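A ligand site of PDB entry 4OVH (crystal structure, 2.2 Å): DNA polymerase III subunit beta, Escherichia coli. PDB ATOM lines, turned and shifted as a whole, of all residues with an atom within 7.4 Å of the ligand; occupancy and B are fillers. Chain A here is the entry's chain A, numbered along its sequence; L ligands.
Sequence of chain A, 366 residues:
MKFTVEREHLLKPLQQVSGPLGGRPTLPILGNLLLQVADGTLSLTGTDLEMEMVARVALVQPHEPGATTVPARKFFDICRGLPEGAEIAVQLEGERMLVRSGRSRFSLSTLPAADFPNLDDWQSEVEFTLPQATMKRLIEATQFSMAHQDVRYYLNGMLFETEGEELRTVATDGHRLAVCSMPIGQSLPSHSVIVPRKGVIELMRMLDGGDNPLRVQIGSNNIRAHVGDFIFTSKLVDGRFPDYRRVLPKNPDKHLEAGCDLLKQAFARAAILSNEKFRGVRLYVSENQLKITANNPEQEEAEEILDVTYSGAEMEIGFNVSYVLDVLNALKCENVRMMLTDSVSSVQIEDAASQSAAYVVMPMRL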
ATOM      1  N   ASP A 150      -0.045 -10.996   4.703  1.00  0.00           N
ATOM      2  CA  ASP A 150      -0.004  -9.655   5.301  1.00  0.00           C
ATOM      3  C   ASP A 150      -0.782  -9.639   6.631  1.00  0.00           C
ATOM      4  O   ASP A 150      -1.764 -10.384   6.786  1.00  0.00           O
ATOM      5  CB  ASP A 150      -0.595  -8.634   4.330  1.00  0.00           C
ATOM      6  CG  ASP A 150      -0.200  -7.204   4.658  1.00  0.00           C
ATOM      7  OD1 ASP A 150      -0.740  -6.636   5.639  1.00  0.00           O
ATOM      8  OD2 ASP A 150       0.653  -6.642   3.943  1.00  0.00           O
ATOM      9  N   ARG A 152      -2.669  -7.376   7.545  1.00  0.00           N
ATOM     10  CA  ARG A 152      -4.011  -6.971   7.143  1.00  0.00           C
ATOM     11  C   ARG A 152      -4.644  -8.163   6.435  1.00  0.00           C
ATOM     12  O   ARG A 152      -4.525  -8.313   5.225  1.00  0.00           O
ATOM     13  CB  ARG A 152      -3.985  -5.752   6.219  1.00  0.00           C
ATOM     14  CG  ARG A 152      -3.474  -4.484   6.901  1.00  0.00           C
ATOM     15  CD  ARG A 152      -2.102  -4.102   6.383  1.00  0.00           C
ATOM     16  NE  ARG A 152      -2.184  -3.175   5.267  1.00  0.00           N
ATOM     17  CZ  ARG A 152      -1.248  -3.004   4.339  1.00  0.00           C
ATOM     18  NH1 ARG A 152      -0.145  -3.739   4.317  1.00  0.00           N
ATOM     19  NH2 ARG A 152      -1.449  -2.096   3.392  1.00  0.00           N
ATOM     20  N   TYR A 154      -7.529  -8.855   5.569  1.00  0.00           N
ATOM     21  CA  TYR A 154      -8.495  -8.509   4.498  1.00  0.00           C
ATOM     22  C   TYR A 154      -7.851  -8.395   3.086  1.00  0.00           C
ATOM     23  O   TYR A 154      -8.557  -8.532   2.074  1.00  0.00           O
ATOM     24  CB  TYR A 154      -9.309  -7.253   4.853  1.00  0.00           C
ATOM     25  CG  TYR A 154      -8.508  -5.992   5.176  1.00  0.00           C
ATOM     26  CD1 TYR A 154      -8.179  -5.082   4.168  1.00  0.00           C
ATOM     27  CD2 TYR A 154      -8.122  -5.704   6.492  1.00  0.00           C
ATOM     28  CE1 TYR A 154      -7.443  -3.923   4.466  1.00  0.00           C
ATOM     29  CE2 TYR A 154      -7.386  -4.565   6.788  1.00  0.00           C
ATOM     30  CZ  TYR A 154      -7.045  -3.684   5.774  1.00  0.00           C
ATOM     31  OH  TYR A 154      -6.328  -2.536   6.077  1.00  0.00           O
ATOM     32  N   LEU A 155      -6.543  -8.172   3.017  1.00  0.00           N
ATOM     33  CA  LEU A 155      -5.795  -8.084   1.747  1.00  0.00           C
ATOM     34  C   LEU A 155      -5.311  -9.444   1.216  1.00  0.00           C
ATOM     35  O   LEU A 155      -4.894  -9.532   0.052  1.00  0.00           O
ATOM     36  CB  LEU A 155      -4.571  -7.170   1.898  1.00  0.00           C
ATOM     37  CG  LEU A 155      -4.805  -5.681   2.231  1.00  0.00           C
ATOM     38  CD1 LEU A 155      -3.486  -4.935   2.158  1.00  0.00           C
ATOM     39  CD2 LEU A 155      -5.816  -5.045   1.279  1.00  0.00           C
ATOM     40  N   THR A 172      -5.250  -6.222  -3.947  1.00  0.00           N
ATOM     41  CA  THR A 172      -4.158  -5.291  -3.716  1.00  0.00           C
ATOM     42  C   THR A 172      -3.381  -5.807  -2.524  1.00  0.00           C
ATOM     43  O   THR A 172      -3.952  -6.496  -1.672  1.00  0.00           O
ATOM     44  CB  THR A 172      -4.666  -3.861  -3.449  1.00  0.00           C
ATOM     45  OG1 THR A 172      -3.553  -2.968  -3.227  1.00  0.00           O
ATOM     46  CG2 THR A 172      -5.585  -3.793  -2.236  1.00  0.00           C
ATOM     47  N   ASP A 173      -2.095  -5.493  -2.484  1.00  0.00           N
ATOM     48  CA  ASP A 173      -1.260  -5.852  -1.336  1.00  0.00           C
ATOM     49  C   ASP A 173      -0.740  -4.618  -0.606  1.00  0.00           C
ATOM     50  O   ASP A 173       0.084  -4.737   0.295  1.00  0.00           O
ATOM     51  CB  ASP A 173      -0.098  -6.763  -1.772  1.00  0.00           C
ATOM     52  CG  ASP A 173       0.758  -6.159  -2.890  1.00  0.00           C
ATOM     53  OD1 ASP A 173       0.643  -4.946  -3.190  1.00  0.00           O
ATOM     54  OD2 ASP A 173       1.553  -6.927  -3.464  1.00  0.00           O
ATOM     55  N   GLY A 174      -1.239  -3.447  -1.006  1.00  0.00           N
ATOM     56  CA  GLY A 174      -0.777  -2.172  -0.434  1.00  0.00           C
ATOM     57  C   GLY A 174       0.265  -1.461  -1.272  1.00  0.00           C
ATOM     58  O   GLY A 174       0.484  -0.257  -1.107  1.00  0.00           O
ATOM     59  N   HIS A 175       0.923  -2.190  -2.167  1.00  0.00           N
ATOM     60  CA  HIS A 175       1.937  -1.617  -3.056  1.00  0.00           C
ATOM     61  C   HIS A 175       1.420  -1.482  -4.469  1.00  0.00           C
ATOM     62  O   HIS A 175       1.748  -0.516  -5.165  1.00  0.00           O
ATOM     63  CB  HIS A 175       3.189  -2.488  -3.043  1.00  0.00           C
ATOM     64  CG  HIS A 175       3.760  -2.697  -1.675  1.00  0.00           C
ATOM     65  ND1 HIS A 175       3.783  -3.929  -1.067  1.00  0.00           N
ATOM     66  CD2 HIS A 175       4.279  -1.816  -0.786  1.00  0.00           C
ATOM     67  CE1 HIS A 175       4.315  -3.806   0.144  1.00  0.00           C
ATOM     68  NE2 HIS A 175       4.622  -2.530   0.336  1.00  0.00           N
ATOM     69  N   ARG A 176       0.612  -2.443  -4.899  1.00  0.00           N
ATOM     70  CA  ARG A 176      -0.016  -2.411  -6.226  1.00  0.00           C
ATOM     71  C   ARG A 176      -1.443  -2.952  -6.145  1.00  0.00           C
ATOM     72  O   ARG A 176      -1.809  -3.582  -5.149  1.00  0.00           O
ATOM     73  CB  ARG A 176       0.822  -3.172  -7.250  1.00  0.00           C
ATOM     74  CG  ARG A 176       1.547  -4.411  -6.732  1.00  0.00           C
ATOM     75  CD  ARG A 176       0.613  -5.601  -6.632  1.00  0.00           C
ATOM     76  NE  ARG A 176       1.283  -6.818  -6.178  1.00  0.00           N
ATOM     77  CZ  ARG A 176       2.004  -7.635  -6.941  1.00  0.00           C
ATOM     78  NH1 ARG A 176       2.186  -7.393  -8.245  1.00  0.00           N
ATOM     79  NH2 ARG A 176       2.544  -8.715  -6.401  1.00  0.00           N
ATOM     80  N   LEU A 177      -2.249  -2.692  -7.171  1.00  0.00           N
ATOM     81  CA  LEU A 177      -3.664  -3.073  -7.201  1.00  0.00           C
ATOM     82  C   LEU A 177      -4.108  -3.469  -8.588  1.00  0.00           C
ATOM     83  O   LEU A 177      -3.613  -2.942  -9.603  1.00  0.00           O
ATOM     84  CB  LEU A 177      -4.548  -1.934  -6.680  1.00  0.00           C
ATOM     85  CG  LEU A 177      -6.080  -2.087  -6.750  1.00  0.00           C
ATOM     86  CD1 LEU A 177      -6.756  -1.454  -5.536  1.00  0.00           C
ATOM     87  CD2 LEU A 177      -6.663  -1.503  -8.039  1.00  0.00           C
ATOM     88  N   ALA A 178      -5.038  -4.417  -8.633  1.00  0.00           N
ATOM     89  CA  ALA A 178      -5.677  -4.855  -9.857  1.00  0.00           C
ATOM     90  C   ALA A 178      -7.200  -4.868  -9.657  1.00  0.00           C
ATOM     91  O   ALA A 178      -7.680  -5.307  -8.609  1.00  0.00           O
ATOM     92  CB  ALA A 178      -5.164  -6.237 -10.219  1.00  0.00           C
ATOM     93  N   ARG A 240     -12.544  -4.106   6.544  1.00  0.00           N
ATOM     94  CA  ARG A 240     -12.883  -3.156   5.489  1.00  0.00           C
ATOM     95  C   ARG A 240     -11.808  -3.127   4.407  1.00  0.00           C
ATOM     96  O   ARG A 240     -10.700  -2.635   4.617  1.00  0.00           O
ATOM     97  CB  ARG A 240     -13.043  -1.742   6.046  1.00  0.00           C
ATOM     98  CG  ARG A 240     -14.181  -1.556   7.025  1.00  0.00           C
ATOM     99  CD  ARG A 240     -14.489  -0.089   7.202  1.00  0.00           C
ATOM    100  NE  ARG A 240     -13.282   0.708   7.428  1.00  0.00           N
ATOM    101  CZ  ARG A 240     -12.598   0.744   8.569  1.00  0.00           C
ATOM    102  NH1 ARG A 240     -12.958   0.010   9.619  1.00  0.00           N
ATOM    103  NH2 ARG A 240     -11.512   1.506   8.654  1.00  0.00           N
ATOM    104  N   PHE A 241     -12.180  -3.646   3.232  1.00  0.00           N
ATOM    105  CA  PHE A 241     -11.320  -3.662   2.075  1.00  0.00           C
ATOM    106  C   PHE A 241     -11.213  -2.229   1.550  1.00  0.00           C
ATOM    107  O   PHE A 241     -12.179  -1.471   1.631  1.00  0.00           O
ATOM    108  CB  PHE A 241     -11.918  -4.593   1.009  1.00  0.00           C
ATOM    109  CG  PHE A 241     -10.940  -5.075  -0.006  1.00  0.00           C
ATOM    110  CD1 PHE A 241     -10.137  -6.179   0.248  1.00  0.00           C
ATOM    111  CD2 PHE A 241     -10.827  -4.440  -1.240  1.00  0.00           C
ATOM    112  CE1 PHE A 241      -9.232  -6.631  -0.696  1.00  0.00           C
ATOM    113  CE2 PHE A 241      -9.926  -4.882  -2.193  1.00  0.00           C
ATOM    114  CZ  PHE A 241      -9.126  -5.987  -1.917  1.00  0.00           C
ATOM    115  N   PRO A 242     -10.043  -1.857   1.029  1.00  0.00           N
ATOM    116  CA  PRO A 242      -9.885  -0.517   0.448  1.00  0.00           C
ATOM    117  C   PRO A 242     -10.762  -0.294  -0.790  1.00  0.00           C
ATOM    118  O   PRO A 242     -11.181  -1.248  -1.442  1.00  0.00           O
ATOM    119  CB  PRO A 242      -8.402  -0.471   0.051  1.00  0.00           C
ATOM    120  CG  PRO A 242      -7.971  -1.898  -0.040  1.00  0.00           C
ATOM    121  CD  PRO A 242      -8.788  -2.623   0.983  1.00  0.00           C
ATOM    122  N   ASP A 243     -11.016   0.971  -1.080  1.00  0.00           N
ATOM    123  CA  ASP A 243     -11.862   1.377  -2.189  1.00  0.00           C
ATOM    124  C   ASP A 243     -10.997   1.658  -3.416  1.00  0.00           C
ATOM    125  O   ASP A 243     -10.264   2.654  -3.467  1.00  0.00           O
ATOM    126  CB  ASP A 243     -12.677   2.609  -1.783  1.00  0.00           C
ATOM    127  CG  ASP A 243     -13.486   3.200  -2.926  1.00  0.00           C
ATOM    128  OD1 ASP A 243     -13.358   2.765  -4.082  1.00  0.00           O
ATOM    129  OD2 ASP A 243     -14.250   4.144  -2.651  1.00  0.00           O
ATOM    130  N   VAL A 247      -7.715   4.440  -4.977  1.00  0.00           N
ATOM    131  CA  VAL A 247      -6.400   3.999  -5.418  1.00  0.00           C
ATOM    132  C   VAL A 247      -6.176   4.426  -6.865  1.00  0.00           C
ATOM    133  O   VAL A 247      -5.104   4.900  -7.217  1.00  0.00           O
ATOM    134  CB  VAL A 247      -6.277   2.471  -5.320  1.00  0.00           C
ATOM    135  CG1 VAL A 247      -4.944   2.002  -5.897  1.00  0.00           C
ATOM    136  CG2 VAL A 247      -6.469   2.016  -3.877  1.00  0.00           C
ATOM    137  N   LEU A 248      -7.189   4.229  -7.707  1.00  0.00           N
ATOM    138  CA  LEU A 248      -7.135   4.731  -9.078  1.00  0.00           C
ATOM    139  C   LEU A 248      -6.811   6.213  -9.061  1.00  0.00           C
ATOM    140  O   LEU A 248      -7.352   6.944  -8.229  1.00  0.00           O
ATOM    141  CB  LEU A 248      -8.467   4.549  -9.795  1.00  0.00           C
ATOM    142  CG  LEU A 248      -8.902   3.165 -10.224  1.00  0.00           C
ATOM    143  CD1 LEU A 248     -10.298   3.263 -10.849  1.00  0.00           C
ATOM    144  CD2 LEU A 248      -7.919   2.558 -11.195  1.00  0.00           C
ATOM    145  N   SER A 346       0.578   7.568  -8.204  1.00  0.00           N
ATOM    146  CA  SER A 346       0.373   6.234  -8.754  1.00  0.00           C
ATOM    147  C   SER A 346       0.238   6.297 -10.275  1.00  0.00           C
ATOM    148  O   SER A 346      -0.079   7.341 -10.854  1.00  0.00           O
ATOM    149  CB  SER A 346      -0.864   5.550  -8.132  1.00  0.00           C
ATOM    150  OG  SER A 346      -2.099   6.058  -8.630  1.00  0.00           O
ATOM    151  N   VAL A 347       0.493   5.166 -10.923  1.00  0.00           N
ATOM    152  CA  VAL A 347       0.315   5.049 -12.366  1.00  0.00           C
ATOM    153  C   VAL A 347      -0.698   3.977 -12.677  1.00  0.00           C
ATOM    154  O   VAL A 347      -0.751   2.957 -11.997  1.00  0.00           O
ATOM    155  CB  VAL A 347       1.650   4.739 -13.051  1.00  0.00           C
ATOM    156  CG1 VAL A 347       1.471   4.465 -14.534  1.00  0.00           C
ATOM    157  CG2 VAL A 347       2.587   5.914 -12.813  1.00  0.00           C
ATOM    158  N   TYR A 359      -4.830  -1.564 -13.733  1.00  0.00           N
ATOM    159  CA  TYR A 359      -3.791  -1.897 -12.783  1.00  0.00           C
ATOM    160  C   TYR A 359      -3.175  -0.619 -12.287  1.00  0.00           C
ATOM    161  O   TYR A 359      -2.912   0.281 -13.091  1.00  0.00           O
ATOM    162  CB  TYR A 359      -2.745  -2.773 -13.484  1.00  0.00           C
ATOM    163  CG  TYR A 359      -3.370  -4.052 -13.977  1.00  0.00           C
ATOM    164  CD1 TYR A 359      -3.487  -5.149 -13.130  1.00  0.00           C
ATOM    165  CD2 TYR A 359      -3.908  -4.149 -15.259  1.00  0.00           C
ATOM    166  CE1 TYR A 359      -4.097  -6.321 -13.558  1.00  0.00           C
ATOM    167  CE2 TYR A 359      -4.512  -5.320 -15.700  1.00  0.00           C
ATOM    168  CZ  TYR A 359      -4.603  -6.407 -14.840  1.00  0.00           C
ATOM    169  OH  TYR A 359      -5.207  -7.591 -15.250  1.00  0.00           O
ATOM    170  N   VAL A 360      -2.957  -0.530 -10.977  1.00  0.00           N
ATOM    171  CA  VAL A 360      -2.337   0.649 -10.371  1.00  0.00           C
ATOM    172  C   VAL A 360      -1.080   0.271  -9.597  1.00  0.00           C
ATOM    173  O   VAL A 360      -1.100  -0.676  -8.808  1.00  0.00           O
ATOM    174  CB  VAL A 360      -3.317   1.378  -9.426  1.00  0.00           C
ATOM    175  CG1 VAL A 360      -2.653   2.618  -8.800  1.00  0.00           C
ATOM    176  CG2 VAL A 360      -4.560   1.786 -10.182  1.00  0.00           C
ATOM    177  N   VAL A 361      -0.011   1.027  -9.836  1.00  0.00           N
ATOM    178  CA  VAL A 361       1.282   0.821  -9.192  1.00  0.00           C
ATOM    179  C   VAL A 361       1.815   2.140  -8.621  1.00  0.00           C
ATOM    180  O   VAL A 361       1.770   3.163  -9.277  1.00  0.00           O
ATOM    181  CB  VAL A 361       2.317   0.250 -10.189  1.00  0.00           C
ATOM    182  CG1 VAL A 361       3.548  -0.247  -9.456  1.00  0.00           C
ATOM    183  CG2 VAL A 361       1.697  -0.871 -11.026  1.00  0.00           C
ATOM    184  N   MET A 362       2.352   2.101  -7.400  1.00  0.00           N
ATOM    185  CA  MET A 362       2.952   3.289  -6.787  1.00  0.00           C
ATOM    186  C   MET A 362       4.377   3.511  -7.280  1.00  0.00           C
ATOM    187  O   MET A 362       5.071   2.555  -7.574  1.00  0.00           O
ATOM    188  CB  MET A 362       2.985   3.171  -5.265  1.00  0.00           C
ATOM    189  CG  MET A 362       1.630   3.292  -4.616  1.00  0.00           C
ATOM    190  SD  MET A 362       0.786   4.839  -5.041  1.00  0.00           S
ATOM    191  CE  MET A 362       1.696   6.023  -4.060  1.00  0.00           C
HETATM  192  O1  LIG L   1       2.714  -0.773   2.045  1.00  0.00           O
HETATM  193  C1  LIG L   1       1.523  -0.425   2.213  1.00  0.00           C
HETATM  194  O2  LIG L   1       0.528  -1.176   2.298  1.00  0.00           O
HETATM  195  C2  LIG L   1       1.254   0.993   2.522  1.00  0.00           C
HETATM  196  N1  LIG L   1       0.383   1.601   1.508  1.00  0.00           N
HETATM  197  C3  LIG L   1      -0.248   2.740   1.812  1.00  0.00           C
HETATM  198  O3  LIG L   1       0.032   3.379   2.814  1.00  0.00           O
HETATM  199  C4  LIG L   1      -1.271   3.304   0.870  1.00  0.00           C
HETATM  200  N2  LIG L   1      -2.029   2.153   0.209  1.00  0.00           N
HETATM  201  C5  LIG L   1      -2.882   1.237   0.690  1.00  0.00           C
HETATM  202  C6  LIG L   1      -3.343   1.060   2.002  1.00  0.00           C
HETATM  203  C7  LIG L   1      -4.534   0.052   2.046  1.00  0.00           C
HETATM  204  C8  LIG L   1      -4.855  -0.478   3.467  1.00  0.00           C
HETATM  205  O4  LIG L   1      -3.968  -0.391   4.348  1.00  0.00           O
HETATM  206  O5  LIG L   1      -6.005  -0.961   3.624  1.00  0.00           O
HETATM  207  C9  LIG L   1      -4.243  -1.119   1.159  1.00  0.00           C
HETATM  208  C10 LIG L   1      -4.153  -0.611  -0.256  1.00  0.00           C
HETATM  209  C11 LIG L   1      -3.264   0.467  -0.358  1.00  0.00           C
HETATM  210  C12 LIG L   1      -2.642   0.906  -1.456  1.00  0.00           C
HETATM  211  C13 LIG L   1      -1.887   1.951  -1.098  1.00  0.00           C
HETATM  212  C14 LIG L   1      -1.137   2.602  -1.995  1.00  0.00           C
HETATM  213  C15 LIG L   1      -1.130   2.204  -3.308  1.00  0.00           C
HETATM  214  C16 LIG L   1      -1.904   1.140  -3.692  1.00  0.00           C
HETATM  215 BR1  LIG L   1      -1.801   0.695  -5.499  1.00  0.00          BR
HETATM  216  C17 LIG L   1      -2.674   0.473  -2.736  1.00  0.00           C
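O of Gly 174 lies within hydrogen-bond range of N1 of the ligand, at 3.2 Å. NH2 of Arg 152 is in salt-bridge range of O2 of the ligand (2.4 Å). The side-chain hydroxyl of Tyr 154 sits at hydrogen-bond distance from an oxygen (O5) of the ligand. A ring nitrogen (NE2) of His 175 is in hydrogen-bond range of an oxygen (O1) of the ligand (3.1 Å).
N of Gly 174 is in hydrogen-bond range of OG1 of Thr 172 (3.2 Å). The side-chain carboxylate (OD2) of Asp 173 is in salt-bridge range of the guanidinium group (NE) of Arg 176 (2.7 Å). N of His 175 is in hydrogen-bond range of OD1 of Asp 173 (3.0 Å). The backbone carbonyl oxygen (O) of His 175 sits at hydrogen-bond distance from the backbone NH (N) of Met 362, 3.5 Å away. The guanidinium group of Arg 152 is in salt-bridge range of the side-chain carboxylate of Asp 150 (3.0 Å). OG1 of Thr 172 is in hydrogen-bond range of O of Arg 176. The backbone carbonyl oxygen (O) of Val 360 is in hydrogen-bond range of the backbone NH (N) of Leu 177 (2.8 Å).
Merely in contact with the ligand: Met 362 (3.2 Å), Val 247 (3.4 Å), Thr 172 (3.6 Å), Val 360 (3.6 Å), Arg 176 (3.7 Å), Leu 177 (3.8 Å) and Pro 242 (3.99 Å). 11 residues have an atom within 4 Å of the ligand: Arg 152, Tyr 154, Thr 172, Gly 174, His 175, Arg 176, Leu 177, Pro 242, Val 247, Val 360 and Met 362. The nearest printed residue that does not touch the ligand is Leu 155 (4.02 Å).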
